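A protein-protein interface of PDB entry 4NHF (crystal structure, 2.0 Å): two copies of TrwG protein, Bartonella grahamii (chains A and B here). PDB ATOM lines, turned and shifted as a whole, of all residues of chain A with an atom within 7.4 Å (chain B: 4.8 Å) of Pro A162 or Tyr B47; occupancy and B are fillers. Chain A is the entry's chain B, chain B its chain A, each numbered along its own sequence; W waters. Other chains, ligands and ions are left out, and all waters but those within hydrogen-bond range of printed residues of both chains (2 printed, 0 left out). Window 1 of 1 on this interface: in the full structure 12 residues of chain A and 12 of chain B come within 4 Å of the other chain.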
ATOM      1  N   TYR A  40      -6.310   4.029  22.128  1.00  0.00           N
ATOM      2  CA  TYR A  40      -5.441   2.932  21.735  1.00  0.00           C
ATOM      3  C   TYR A  40      -4.198   2.844  22.598  1.00  0.00           C
ATOM      4  O   TYR A  40      -3.283   2.147  22.252  1.00  0.00           O
ATOM      5  CB  TYR A  40      -5.029   3.109  20.271  1.00  0.00           C
ATOM      6  CG  TYR A  40      -6.110   2.689  19.292  1.00  0.00           C
ATOM      7  CD1 TYR A  40      -6.022   1.499  18.639  1.00  0.00           C
ATOM      8  CD2 TYR A  40      -7.242   3.498  19.058  1.00  0.00           C
ATOM      9  CE1 TYR A  40      -7.018   1.068  17.767  1.00  0.00           C
ATOM     10  CE2 TYR A  40      -8.227   3.102  18.173  1.00  0.00           C
ATOM     11  CZ  TYR A  40      -8.102   1.879  17.513  1.00  0.00           C
ATOM     12  OH  TYR A  40      -9.077   1.414  16.640  1.00  0.00           O
ATOM     13  N   TYR A  47       0.990   9.622  19.038  1.00  0.00           N
ATOM     14  CA  TYR A  47       1.230   9.745  17.591  1.00  0.00           C
ATOM     15  C   TYR A  47       0.168  10.659  17.000  1.00  0.00           C
ATOM     16  O   TYR A  47       0.480  11.643  16.284  1.00  0.00           O
ATOM     17  CB  TYR A  47       1.237   8.386  16.866  1.00  0.00           C
ATOM     18  CG  TYR A  47       1.294   8.573  15.369  1.00  0.00           C
ATOM     19  CD1 TYR A  47       2.504   8.840  14.702  1.00  0.00           C
ATOM     20  CD2 TYR A  47       0.136   8.544  14.618  1.00  0.00           C
ATOM     21  CE1 TYR A  47       2.545   8.996  13.336  1.00  0.00           C
ATOM     22  CE2 TYR A  47       0.178   8.730  13.248  1.00  0.00           C
ATOM     23  CZ  TYR A  47       1.397   8.962  12.632  1.00  0.00           C
ATOM     24  OH  TYR A  47       1.419   9.165  11.300  1.00  0.00           O
ATOM     25  N   TRP A  48      -1.087  10.386  17.298  1.00  0.00           N
ATOM     26  CA  TRP A  48      -2.161  11.160  16.672  1.00  0.00           C
ATOM     27  C   TRP A  48      -2.267  12.598  17.205  1.00  0.00           C
ATOM     28  O   TRP A  48      -2.509  13.535  16.440  1.00  0.00           O
ATOM     29  CB  TRP A  48      -3.520  10.419  16.763  1.00  0.00           C
ATOM     30  CG  TRP A  48      -3.523   9.273  15.833  1.00  0.00           C
ATOM     31  CD1 TRP A  48      -3.381   7.972  16.136  1.00  0.00           C
ATOM     32  CD2 TRP A  48      -3.579   9.356  14.422  1.00  0.00           C
ATOM     33  NE1 TRP A  48      -3.339   7.221  14.981  1.00  0.00           N
ATOM     34  CE2 TRP A  48      -3.503   8.060  13.925  1.00  0.00           C
ATOM     35  CE3 TRP A  48      -3.724  10.413  13.529  1.00  0.00           C
ATOM     36  CZ2 TRP A  48      -3.514   7.789  12.563  1.00  0.00           C
ATOM     37  CZ3 TRP A  48      -3.783  10.131  12.195  1.00  0.00           C
ATOM     38  CH2 TRP A  48      -3.697   8.846  11.727  1.00  0.00           C
ATOM     39  N   GLN A  51       0.526  14.490  15.481  1.00  0.00           N
ATOM     40  CA  GLN A  51       0.192  14.838  14.099  1.00  0.00           C
ATOM     41  C   GLN A  51      -0.899  15.949  14.045  1.00  0.00           C
ATOM     42  O   GLN A  51      -0.860  16.835  13.182  1.00  0.00           O
ATOM     43  CB  GLN A  51      -0.227  13.656  13.243  1.00  0.00           C
ATOM     44  CG  GLN A  51       0.896  12.668  12.920  1.00  0.00           C
ATOM     45  CD  GLN A  51       2.052  13.342  12.218  1.00  0.00           C
ATOM     46  OE1 GLN A  51       1.848  14.064  11.277  1.00  0.00           O
ATOM     47  NE2 GLN A  51       3.253  13.175  12.725  1.00  0.00           N
ATOM     48  N   LEU A  73     -10.333  16.764   9.051  1.00  0.00           N
ATOM     49  CA  LEU A  73     -10.765  15.382   9.084  1.00  0.00           C
ATOM     50  C   LEU A  73     -10.523  14.699  10.459  1.00  0.00           C
ATOM     51  O   LEU A  73     -11.237  13.764  10.854  1.00  0.00           O
ATOM     52  CB  LEU A  73     -10.057  14.676   7.955  1.00  0.00           C
ATOM     53  CG  LEU A  73      -9.984  13.197   8.122  1.00  0.00           C
ATOM     54  CD1 LEU A  73     -11.079  12.605   7.246  1.00  0.00           C
ATOM     55  CD2 LEU A  73      -8.602  12.729   7.758  1.00  0.00           C
ATOM     56  N   LEU A  74      -9.504  15.169  11.190  1.00  0.00           N
ATOM     57  CA  LEU A  74      -9.227  14.717  12.531  1.00  0.00           C
ATOM     58  C   LEU A  74     -10.043  15.431  13.627  1.00  0.00           C
ATOM     59  O   LEU A  74      -9.828  15.182  14.820  1.00  0.00           O
ATOM     60  CB  LEU A  74      -7.731  14.866  12.813  1.00  0.00           C
ATOM     61  CG  LEU A  74      -6.781  14.091  11.888  1.00  0.00           C
ATOM     62  CD1 LEU A  74      -5.394  14.175  12.464  1.00  0.00           C
ATOM     63  CD2 LEU A  74      -7.127  12.626  11.773  1.00  0.00           C
ATOM     64  N   TYR A 148     -11.715   8.113  19.546  1.00  0.00           N
ATOM     65  CA  TYR A 148     -11.665   7.447  18.275  1.00  0.00           C
ATOM     66  C   TYR A 148     -13.035   6.899  17.962  1.00  0.00           C
ATOM     67  O   TYR A 148     -13.710   6.332  18.851  1.00  0.00           O
ATOM     68  CB  TYR A 148     -10.713   6.297  18.372  1.00  0.00           C
ATOM     69  CG  TYR A 148      -9.251   6.604  18.648  1.00  0.00           C
ATOM     70  CD1 TYR A 148      -8.787   6.783  19.936  1.00  0.00           C
ATOM     71  CD2 TYR A 148      -8.333   6.713  17.602  1.00  0.00           C
ATOM     72  CE1 TYR A 148      -7.433   7.025  20.184  1.00  0.00           C
ATOM     73  CE2 TYR A 148      -6.992   6.923  17.840  1.00  0.00           C
ATOM     74  CZ  TYR A 148      -6.547   7.067  19.123  1.00  0.00           C
ATOM     75  OH  TYR A 148      -5.223   7.296  19.324  1.00  0.00           O
ATOM     76  N   GLY A 150     -13.823   5.041  14.885  1.00  0.00           N
ATOM     77  CA  GLY A 150     -13.831   3.964  13.877  1.00  0.00           C
ATOM     78  C   GLY A 150     -13.538   4.500  12.482  1.00  0.00           C
ATOM     79  O   GLY A 150     -13.629   5.680  12.231  1.00  0.00           O
ATOM     80  N   ALA A 151     -13.239   3.597  11.556  1.00  0.00           N
ATOM     81  CA  ALA A 151     -12.809   3.950  10.216  1.00  0.00           C
ATOM     82  C   ALA A 151     -13.858   4.783   9.528  1.00  0.00           C
ATOM     83  O   ALA A 151     -14.997   4.401   9.519  1.00  0.00           O
ATOM     84  CB  ALA A 151     -12.580   2.681   9.403  1.00  0.00           C
ATOM     85  N   PRO A 152     -13.484   5.900   8.913  1.00  0.00           N
ATOM     86  CA  PRO A 152     -14.462   6.639   8.113  1.00  0.00           C
ATOM     87  C   PRO A 152     -14.948   5.848   6.902  1.00  0.00           C
ATOM     88  O   PRO A 152     -14.221   5.006   6.411  1.00  0.00           O
ATOM     89  CB  PRO A 152     -13.690   7.883   7.646  1.00  0.00           C
ATOM     90  CG  PRO A 152     -12.502   7.966   8.516  1.00  0.00           C
ATOM     91  CD  PRO A 152     -12.210   6.595   9.034  1.00  0.00           C
ATOM     92  N   ASP A 157     -10.744   9.846   3.273  1.00  0.00           N
ATOM     93  CA  ASP A 157     -10.704  10.095   4.700  1.00  0.00           C
ATOM     94  C   ASP A 157     -10.110   8.886   5.450  1.00  0.00           C
ATOM     95  O   ASP A 157      -9.281   9.035   6.363  1.00  0.00           O
ATOM     96  CB  ASP A 157     -12.126  10.317   5.217  1.00  0.00           C
ATOM     97  CG  ASP A 157     -12.799  11.588   4.646  1.00  0.00           C
ATOM     98  OD1 ASP A 157     -12.083  12.447   4.106  1.00  0.00           O
ATOM     99  OD2 ASP A 157     -14.046  11.728   4.775  1.00  0.00           O
ATOM    100  N   ARG A 158     -10.567   7.702   5.083  1.00  0.00           N
ATOM    101  CA  ARG A 158     -10.075   6.466   5.684  1.00  0.00           C
ATOM    102  C   ARG A 158      -8.552   6.318   5.457  1.00  0.00           C
ATOM    103  O   ARG A 158      -7.825   5.876   6.335  1.00  0.00           O
ATOM    104  CB  ARG A 158     -10.872   5.276   5.147  1.00  0.00           C
ATOM    105  CG  ARG A 158     -10.675   4.005   5.952  1.00  0.00           C
ATOM    106  CD  ARG A 158     -11.650   2.902   5.573  1.00  0.00           C
ATOM    107  NE  ARG A 158     -11.731   2.767   4.134  1.00  0.00           N
ATOM    108  CZ  ARG A 158     -12.753   3.177   3.380  1.00  0.00           C
ATOM    109  NH1 ARG A 158     -12.720   3.011   2.052  1.00  0.00           N
ATOM    110  NH2 ARG A 158     -13.835   3.731   3.926  1.00  0.00           N
ATOM    111  N   LEU A 159      -8.075   6.794   4.310  1.00  0.00           N
ATOM    112  CA  LEU A 159      -6.667   6.748   3.972  1.00  0.00           C
ATOM    113  C   LEU A 159      -5.814   7.573   4.867  1.00  0.00           C
ATOM    114  O   LEU A 159      -4.654   7.233   5.065  1.00  0.00           O
ATOM    115  CB  LEU A 159      -6.444   7.217   2.535  1.00  0.00           C
ATOM    116  CG  LEU A 159      -5.131   6.829   1.836  1.00  0.00           C
ATOM    117  CD1 LEU A 159      -4.880   5.332   1.908  1.00  0.00           C
ATOM    118  CD2 LEU A 159      -5.124   7.300   0.396  1.00  0.00           C
ATOM    119  N   LEU A 160      -6.365   8.682   5.381  1.00  0.00           N
ATOM    120  CA  LEU A 160      -5.671   9.587   6.249  1.00  0.00           C
ATOM    121  C   LEU A 160      -6.030   9.496   7.720  1.00  0.00           C
ATOM    122  O   LEU A 160      -5.350  10.115   8.542  1.00  0.00           O
ATOM    123  CB  LEU A 160      -5.903  11.028   5.787  1.00  0.00           C
ATOM    124  CG  LEU A 160      -5.397  11.346   4.385  1.00  0.00           C
ATOM    125  CD1 LEU A 160      -5.746  12.768   4.037  1.00  0.00           C
ATOM    126  CD2 LEU A 160      -3.889  11.193   4.412  1.00  0.00           C
ATOM    127  N   ASN A 161      -7.043   8.723   8.079  1.00  0.00           N
ATOM    128  CA  ASN A 161      -7.487   8.622   9.482  1.00  0.00           C
ATOM    129  C   ASN A 161      -8.068   7.256   9.683  1.00  0.00           C
ATOM    130  O   ASN A 161      -9.257   7.096   9.902  1.00  0.00           O
ATOM    131  CB  ASN A 161      -8.456   9.732   9.840  1.00  0.00           C
ATOM    132  CG  ASN A 161      -8.868   9.745  11.319  1.00  0.00           C
ATOM    133  OD1 ASN A 161      -8.221   9.145  12.207  1.00  0.00           O
ATOM    134  ND2 ASN A 161      -9.986  10.421  11.577  1.00  0.00           N
ATOM    135  N   PRO A 162      -7.204   6.252   9.619  1.00  0.00           N
ATOM    136  CA  PRO A 162      -7.652   4.878   9.619  1.00  0.00           C
ATOM    137  C   PRO A 162      -8.437   4.425  10.845  1.00  0.00           C
ATOM    138  O   PRO A 162      -9.303   3.558  10.698  1.00  0.00           O
ATOM    139  CB  PRO A 162      -6.350   4.100   9.565  1.00  0.00           C
ATOM    140  CG  PRO A 162      -5.322   5.021  10.061  1.00  0.00           C
ATOM    141  CD  PRO A 162      -5.732   6.337   9.529  1.00  0.00           C
ATOM    142  N   LEU A 163      -8.119   4.957  12.022  1.00  0.00           N
ATOM    143  CA  LEU A 163      -8.829   4.588  13.277  1.00  0.00           C
ATOM    144  C   LEU A 163     -10.000   5.537  13.620  1.00  0.00           C
ATOM    145  O   LEU A 163     -10.666   5.327  14.642  1.00  0.00           O
ATOM    146  CB  LEU A 163      -7.848   4.583  14.451  1.00  0.00           C
ATOM    147  CG  LEU A 163      -6.522   3.859  14.178  1.00  0.00           C
ATOM    148  CD1 LEU A 163      -5.622   3.980  15.400  1.00  0.00           C
ATOM    149  CD2 LEU A 163      -6.747   2.407  13.817  1.00  0.00           C
ATOM    150  N   GLY A 164     -10.208   6.575  12.812  1.00  0.00           N
ATOM    151  CA  GLY A 164     -11.173   7.655  13.127  1.00  0.00           C
ATOM    152  C   GLY A 164     -10.844   8.393  14.415  1.00  0.00           C
ATOM    153  O   GLY A 164     -11.727   8.560  15.322  1.00  0.00           O
ATOM    154  N   PHE A 165      -9.575   8.768  14.549  1.00  0.00           N
ATOM    155  CA  PHE A 165      -9.167   9.679  15.592  1.00  0.00           C
ATOM    156  C   PHE A 165      -9.968  10.968  15.446  1.00  0.00           C
ATOM    157  O   PHE A 165     -10.156  11.485  14.325  1.00  0.00           O
ATOM    158  CB  PHE A 165      -7.673   9.912  15.503  1.00  0.00           C
ATOM    159  CG  PHE A 165      -7.120  10.885  16.509  1.00  0.00           C
ATOM    160  CD1 PHE A 165      -6.927  10.519  17.820  1.00  0.00           C
ATOM    161  CD2 PHE A 165      -6.766  12.171  16.105  1.00  0.00           C
ATOM    162  CE1 PHE A 165      -6.359  11.402  18.734  1.00  0.00           C
ATOM    163  CE2 PHE A 165      -6.240  13.067  17.010  1.00  0.00           C
ATOM    164  CZ  PHE A 165      -6.017  12.690  18.325  1.00  0.00           C
ATOM    165  N   VAL B  43      -6.748  -1.502   6.221  1.00  0.00           N
ATOM    166  CA  VAL B  43      -6.964  -0.065   6.449  1.00  0.00           C
ATOM    167  C   VAL B  43      -5.700   0.597   7.030  1.00  0.00           C
ATOM    168  O   VAL B  43      -5.240   1.663   6.589  1.00  0.00           O
ATOM    169  CB  VAL B  43      -8.218   0.132   7.340  1.00  0.00           C
ATOM    170  CG1 VAL B  43      -8.330   1.514   7.832  1.00  0.00           C
ATOM    171  CG2 VAL B  43      -9.463  -0.199   6.529  1.00  0.00           C
ATOM    172  N   VAL B  44      -5.104  -0.075   7.994  1.00  0.00           N
ATOM    173  CA  VAL B  44      -3.914   0.412   8.630  1.00  0.00           C
ATOM    174  C   VAL B  44      -2.699   0.328   7.644  1.00  0.00           C
ATOM    175  O   VAL B  44      -1.898   1.302   7.550  1.00  0.00           O
ATOM    176  CB  VAL B  44      -3.651  -0.330   9.954  1.00  0.00           C
ATOM    177  CG1 VAL B  44      -2.303  -0.009  10.563  1.00  0.00           C
ATOM    178  CG2 VAL B  44      -4.784  -0.080  10.994  1.00  0.00           C
ATOM    179  N   ASP B  45      -2.572  -0.781   6.893  1.00  0.00           N
ATOM    180  CA  ASP B  45      -1.485  -0.904   5.920  1.00  0.00           C
ATOM    181  C   ASP B  45      -1.532   0.204   4.881  1.00  0.00           C
ATOM    182  O   ASP B  45      -0.523   0.781   4.584  1.00  0.00           O
ATOM    183  CB  ASP B  45      -1.480  -2.229   5.177  1.00  0.00           C
ATOM    184  CG  ASP B  45      -1.216  -3.442   6.077  1.00  0.00           C
ATOM    185  OD1 ASP B  45      -0.763  -3.340   7.224  1.00  0.00           O
ATOM    186  OD2 ASP B  45      -1.354  -4.513   5.527  1.00  0.00           O
ATOM    187  N   ARG B  46      -2.714   0.486   4.335  1.00  0.00           N
ATOM    188  CA  ARG B  46      -2.882   1.513   3.357  1.00  0.00           C
ATOM    189  C   ARG B  46      -2.473   2.867   3.901  1.00  0.00           C
ATOM    190  O   ARG B  46      -1.814   3.647   3.189  1.00  0.00           O
ATOM    191  CB  ARG B  46      -4.332   1.544   2.834  1.00  0.00           C
ATOM    192  CG  ARG B  46      -4.649   0.446   1.824  1.00  0.00           C
ATOM    193  CD  ARG B  46      -6.014   0.613   1.124  1.00  0.00           C
ATOM    194  NE  ARG B  46      -5.919  -0.209  -0.104  1.00  0.00           N
ATOM    195  CZ  ARG B  46      -6.249  -1.502  -0.161  1.00  0.00           C
ATOM    196  NH1 ARG B  46      -6.118  -2.185  -1.296  1.00  0.00           N
ATOM    197  NH2 ARG B  46      -6.782  -2.114   0.923  1.00  0.00           N
ATOM    198  N   TYR B  47      -2.874   3.182   5.139  1.00  0.00           N
ATOM    199  CA  TYR B  47      -2.385   4.390   5.792  1.00  0.00           C
ATOM    200  C   TYR B  47      -0.866   4.564   5.696  1.00  0.00           C
ATOM    201  O   TYR B  47      -0.347   5.593   5.179  1.00  0.00           O
ATOM    202  CB  TYR B  47      -2.842   4.486   7.268  1.00  0.00           C
ATOM    203  CG  TYR B  47      -2.283   5.709   7.920  1.00  0.00           C
ATOM    204  CD1 TYR B  47      -2.837   6.978   7.676  1.00  0.00           C
ATOM    205  CD2 TYR B  47      -1.194   5.621   8.750  1.00  0.00           C
ATOM    206  CE1 TYR B  47      -2.286   8.108   8.243  1.00  0.00           C
ATOM    207  CE2 TYR B  47      -0.635   6.756   9.314  1.00  0.00           C
ATOM    208  CZ  TYR B  47      -1.195   7.993   9.069  1.00  0.00           C
ATOM    209  OH  TYR B  47      -0.656   9.092   9.640  1.00  0.00           O
ATOM    210  N   TRP B  48      -0.148   3.572   6.188  1.00  0.00           N
ATOM    211  CA  TRP B  48       1.305   3.643   6.289  1.00  0.00           C
ATOM    212  C   TRP B  48       1.999   3.558   4.929  1.00  0.00           C
ATOM    213  O   TRP B  48       2.992   4.262   4.674  1.00  0.00           O
ATOM    214  CB  TRP B  48       1.815   2.577   7.276  1.00  0.00           C
ATOM    215  CG  TRP B  48       1.502   2.938   8.653  1.00  0.00           C
ATOM    216  CD1 TRP B  48       0.561   2.358   9.468  1.00  0.00           C
ATOM    217  CD2 TRP B  48       2.085   3.983   9.405  1.00  0.00           C
ATOM    218  NE1 TRP B  48       0.513   3.010  10.675  1.00  0.00           N
ATOM    219  CE2 TRP B  48       1.451   4.006  10.658  1.00  0.00           C
ATOM    220  CE3 TRP B  48       3.054   4.939   9.128  1.00  0.00           C
ATOM    221  CZ2 TRP B  48       1.778   4.937  11.638  1.00  0.00           C
ATOM    222  CZ3 TRP B  48       3.407   5.834  10.118  1.00  0.00           C
ATOM    223  CH2 TRP B  48       2.770   5.824  11.354  1.00  0.00           C
ATOM    224  N   LEU B  49       1.472   2.738   4.018  1.00  0.00           N
ATOM    225  CA  LEU B  49       2.070   2.654   2.687  1.00  0.00           C
ATOM    226  C   LEU B  49       1.918   3.977   1.946  1.00  0.00           C
ATOM    227  O   LEU B  49       2.841   4.396   1.249  1.00  0.00           O
ATOM    228  CB  LEU B  49       1.466   1.533   1.857  1.00  0.00           C
ATOM    229  CG  LEU B  49       1.882   0.131   2.354  1.00  0.00           C
ATOM    230  CD1 LEU B  49       0.873  -0.838   1.850  1.00  0.00           C
ATOM    231  CD2 LEU B  49       3.292  -0.267   1.931  1.00  0.00           C
ATOM    232  N   ASN B  50       0.722   4.571   2.028  1.00  0.00           N
ATOM    233  CA  ASN B  50       0.497   5.872   1.485  1.00  0.00           C
ATOM    234  C   ASN B  50       1.421   6.911   2.097  1.00  0.00           C
ATOM    235  O   ASN B  50       2.001   7.733   1.329  1.00  0.00           O
ATOM    236  CB  ASN B  50      -0.971   6.253   1.695  1.00  0.00           C
ATOM    237  CG  ASN B  50      -1.346   7.577   1.053  1.00  0.00           C
ATOM    238  OD1 ASN B  50      -1.226   7.760  -0.158  1.00  0.00           O
ATOM    239  ND2 ASN B  50      -1.863   8.480   1.854  1.00  0.00           N
ATOM    240  N   GLN B  51       1.533   6.963   3.436  1.00  0.00           N
ATOM    241  CA  GLN B  51       2.450   7.961   4.023  1.00  0.00           C
ATOM    242  C   GLN B  51       3.909   7.754   3.511  1.00  0.00           C
ATOM    243  O   GLN B  51       4.644   8.704   3.255  1.00  0.00           O
ATOM    244  CB  GLN B  51       2.408   7.996   5.538  1.00  0.00           C
ATOM    245  CG  GLN B  51       1.126   8.637   6.118  1.00  0.00           C
ATOM    246  CD  GLN B  51       0.884  10.042   5.640  1.00  0.00           C
ATOM    247  OE1 GLN B  51       1.773  10.881   5.718  1.00  0.00           O
ATOM    248  NE2 GLN B  51      -0.264  10.290   5.065  1.00  0.00           N
HETATM  249  O   HOH W   1      -6.321   3.714   5.314  1.00  0.00           O
HETATM  250  O   HOH W   2      -2.064   7.701   4.727  1.00  0.00           O
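The backbone carbonyl oxygen (O) of Pro A152 is in hydrogen-bond range of the guanidinium group (NH2) of Arg A158, 2.8 Å away.
Water W1 lies within hydrogen-bond range of the backbone carbonyl oxygen (O) of Val B43 (2.6 Å), the backbone carbonyl oxygen (O) of Arg A158 (2.8 Å) and the backbone NH (N) of Tyr B47 (3.5 Å).
Water W2 lies within hydrogen-bond range of the backbone carbonyl oxygen (O) of Leu A159 (2.7 Å), the backbone carbonyl oxygen (O) of Tyr B47 (2.8 Å), the side-chain amide nitrogen (ND2) of Asn B50 (3.0 Å) and the side-chain amide nitrogen (NE2) of Gln B51 (3.2 Å).
Printed residues of chain A that touch a printed residue of chain B: Tyr A47, Trp A48, Arg A158, Leu A159, Leu A160 and Pro A162.
Hydrophobic or aromatic side chains of chain A within 4 Å of the printed part of chain B: Tyr A47, Trp A48, Leu A159, Leu A160 and Pro A162.
Hydrophobic or aromatic side chains of chain B within 4 Å of the printed part of chain A: Val B43, Tyr B47 and Trp B48.
Among the printed residues, 11 pairs touch across the chains.
Among the printed residues, no Asp or Glu carboxylate lies within 4 Å of a Lys or Arg side-chain nitrogen of the other chain.
Among the printed residues, merely in contact across the chains: Leu A159 with Tyr B47 (3.2 Å), Pro A162 with Tyr B47 (3.5 Å), Tyr A47 with Trp B48 (3.6 Å), Pro A162 with Val B43 (3.7 Å), Leu A159 with Asn B50 (3.7 Å), Leu A160 with Tyr B47 (3.7 Å), Trp A48 with Tyr B47 (3.7 Å), Leu A159 with Arg B46 (3.7 Å), Leu A160 with Gln B51 (3.8 Å) and Arg A158 with Val B43 (3.9 Å).
Tyr B47 touches its own counterpart, Tyr A47.
Tyr A47 touches Trp B48, and with the chains exchanged Trp A48 touches Tyr B47.
3 positions are printed for both chains.
The side-chain hydroxyl (OH) of Tyr B47 lies within hydrogen-bond range of the side-chain hydroxyl (OH) of Tyr A47, at 2.7 Å.
Of chain B, only Val B43 and Tyr B47 come within 4 Å of Pro A162.
Tyr B47 touches just these residues of chain A: Tyr A47 (2.7 Å), Trp A48 (3.7 Å), Leu A159 (3.2 Å), Leu A160 (3.7 Å) and Pro A162 (3.5 Å).
Of the printed residues of chain B, Tyr A47 touches Tyr B47 and Trp B48.
Of the printed residues of chain B, Leu A159 touches Arg B46 (3.7 Å), Tyr B47 (3.2 Å) and Asn B50 (3.7 Å).
Printed residues of chain A within 4 Å of Val B43: Arg A158 and Pro A162.
Printed residues of chain B within 4 Å of Leu A160: Tyr B47 (3.7 Å) and Gln B51 (3.8 Å).
Of the printed residues of chain A, Arg B46 touches Leu A159.
Phe A165 touches none of the printed residues of chain B.
Leu B49 touches none of the printed residues of chain A.
The nearest residue of chain B that does not touch Pro A162 is Val B44 (4.5 Å).
The nearest residue of chain A that does not touch Tyr B47 is Asn A161 (4.6 Å).
The nearest printed residue of chain A that does not touch Val B43 is Ala A151 (4.7 Å).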
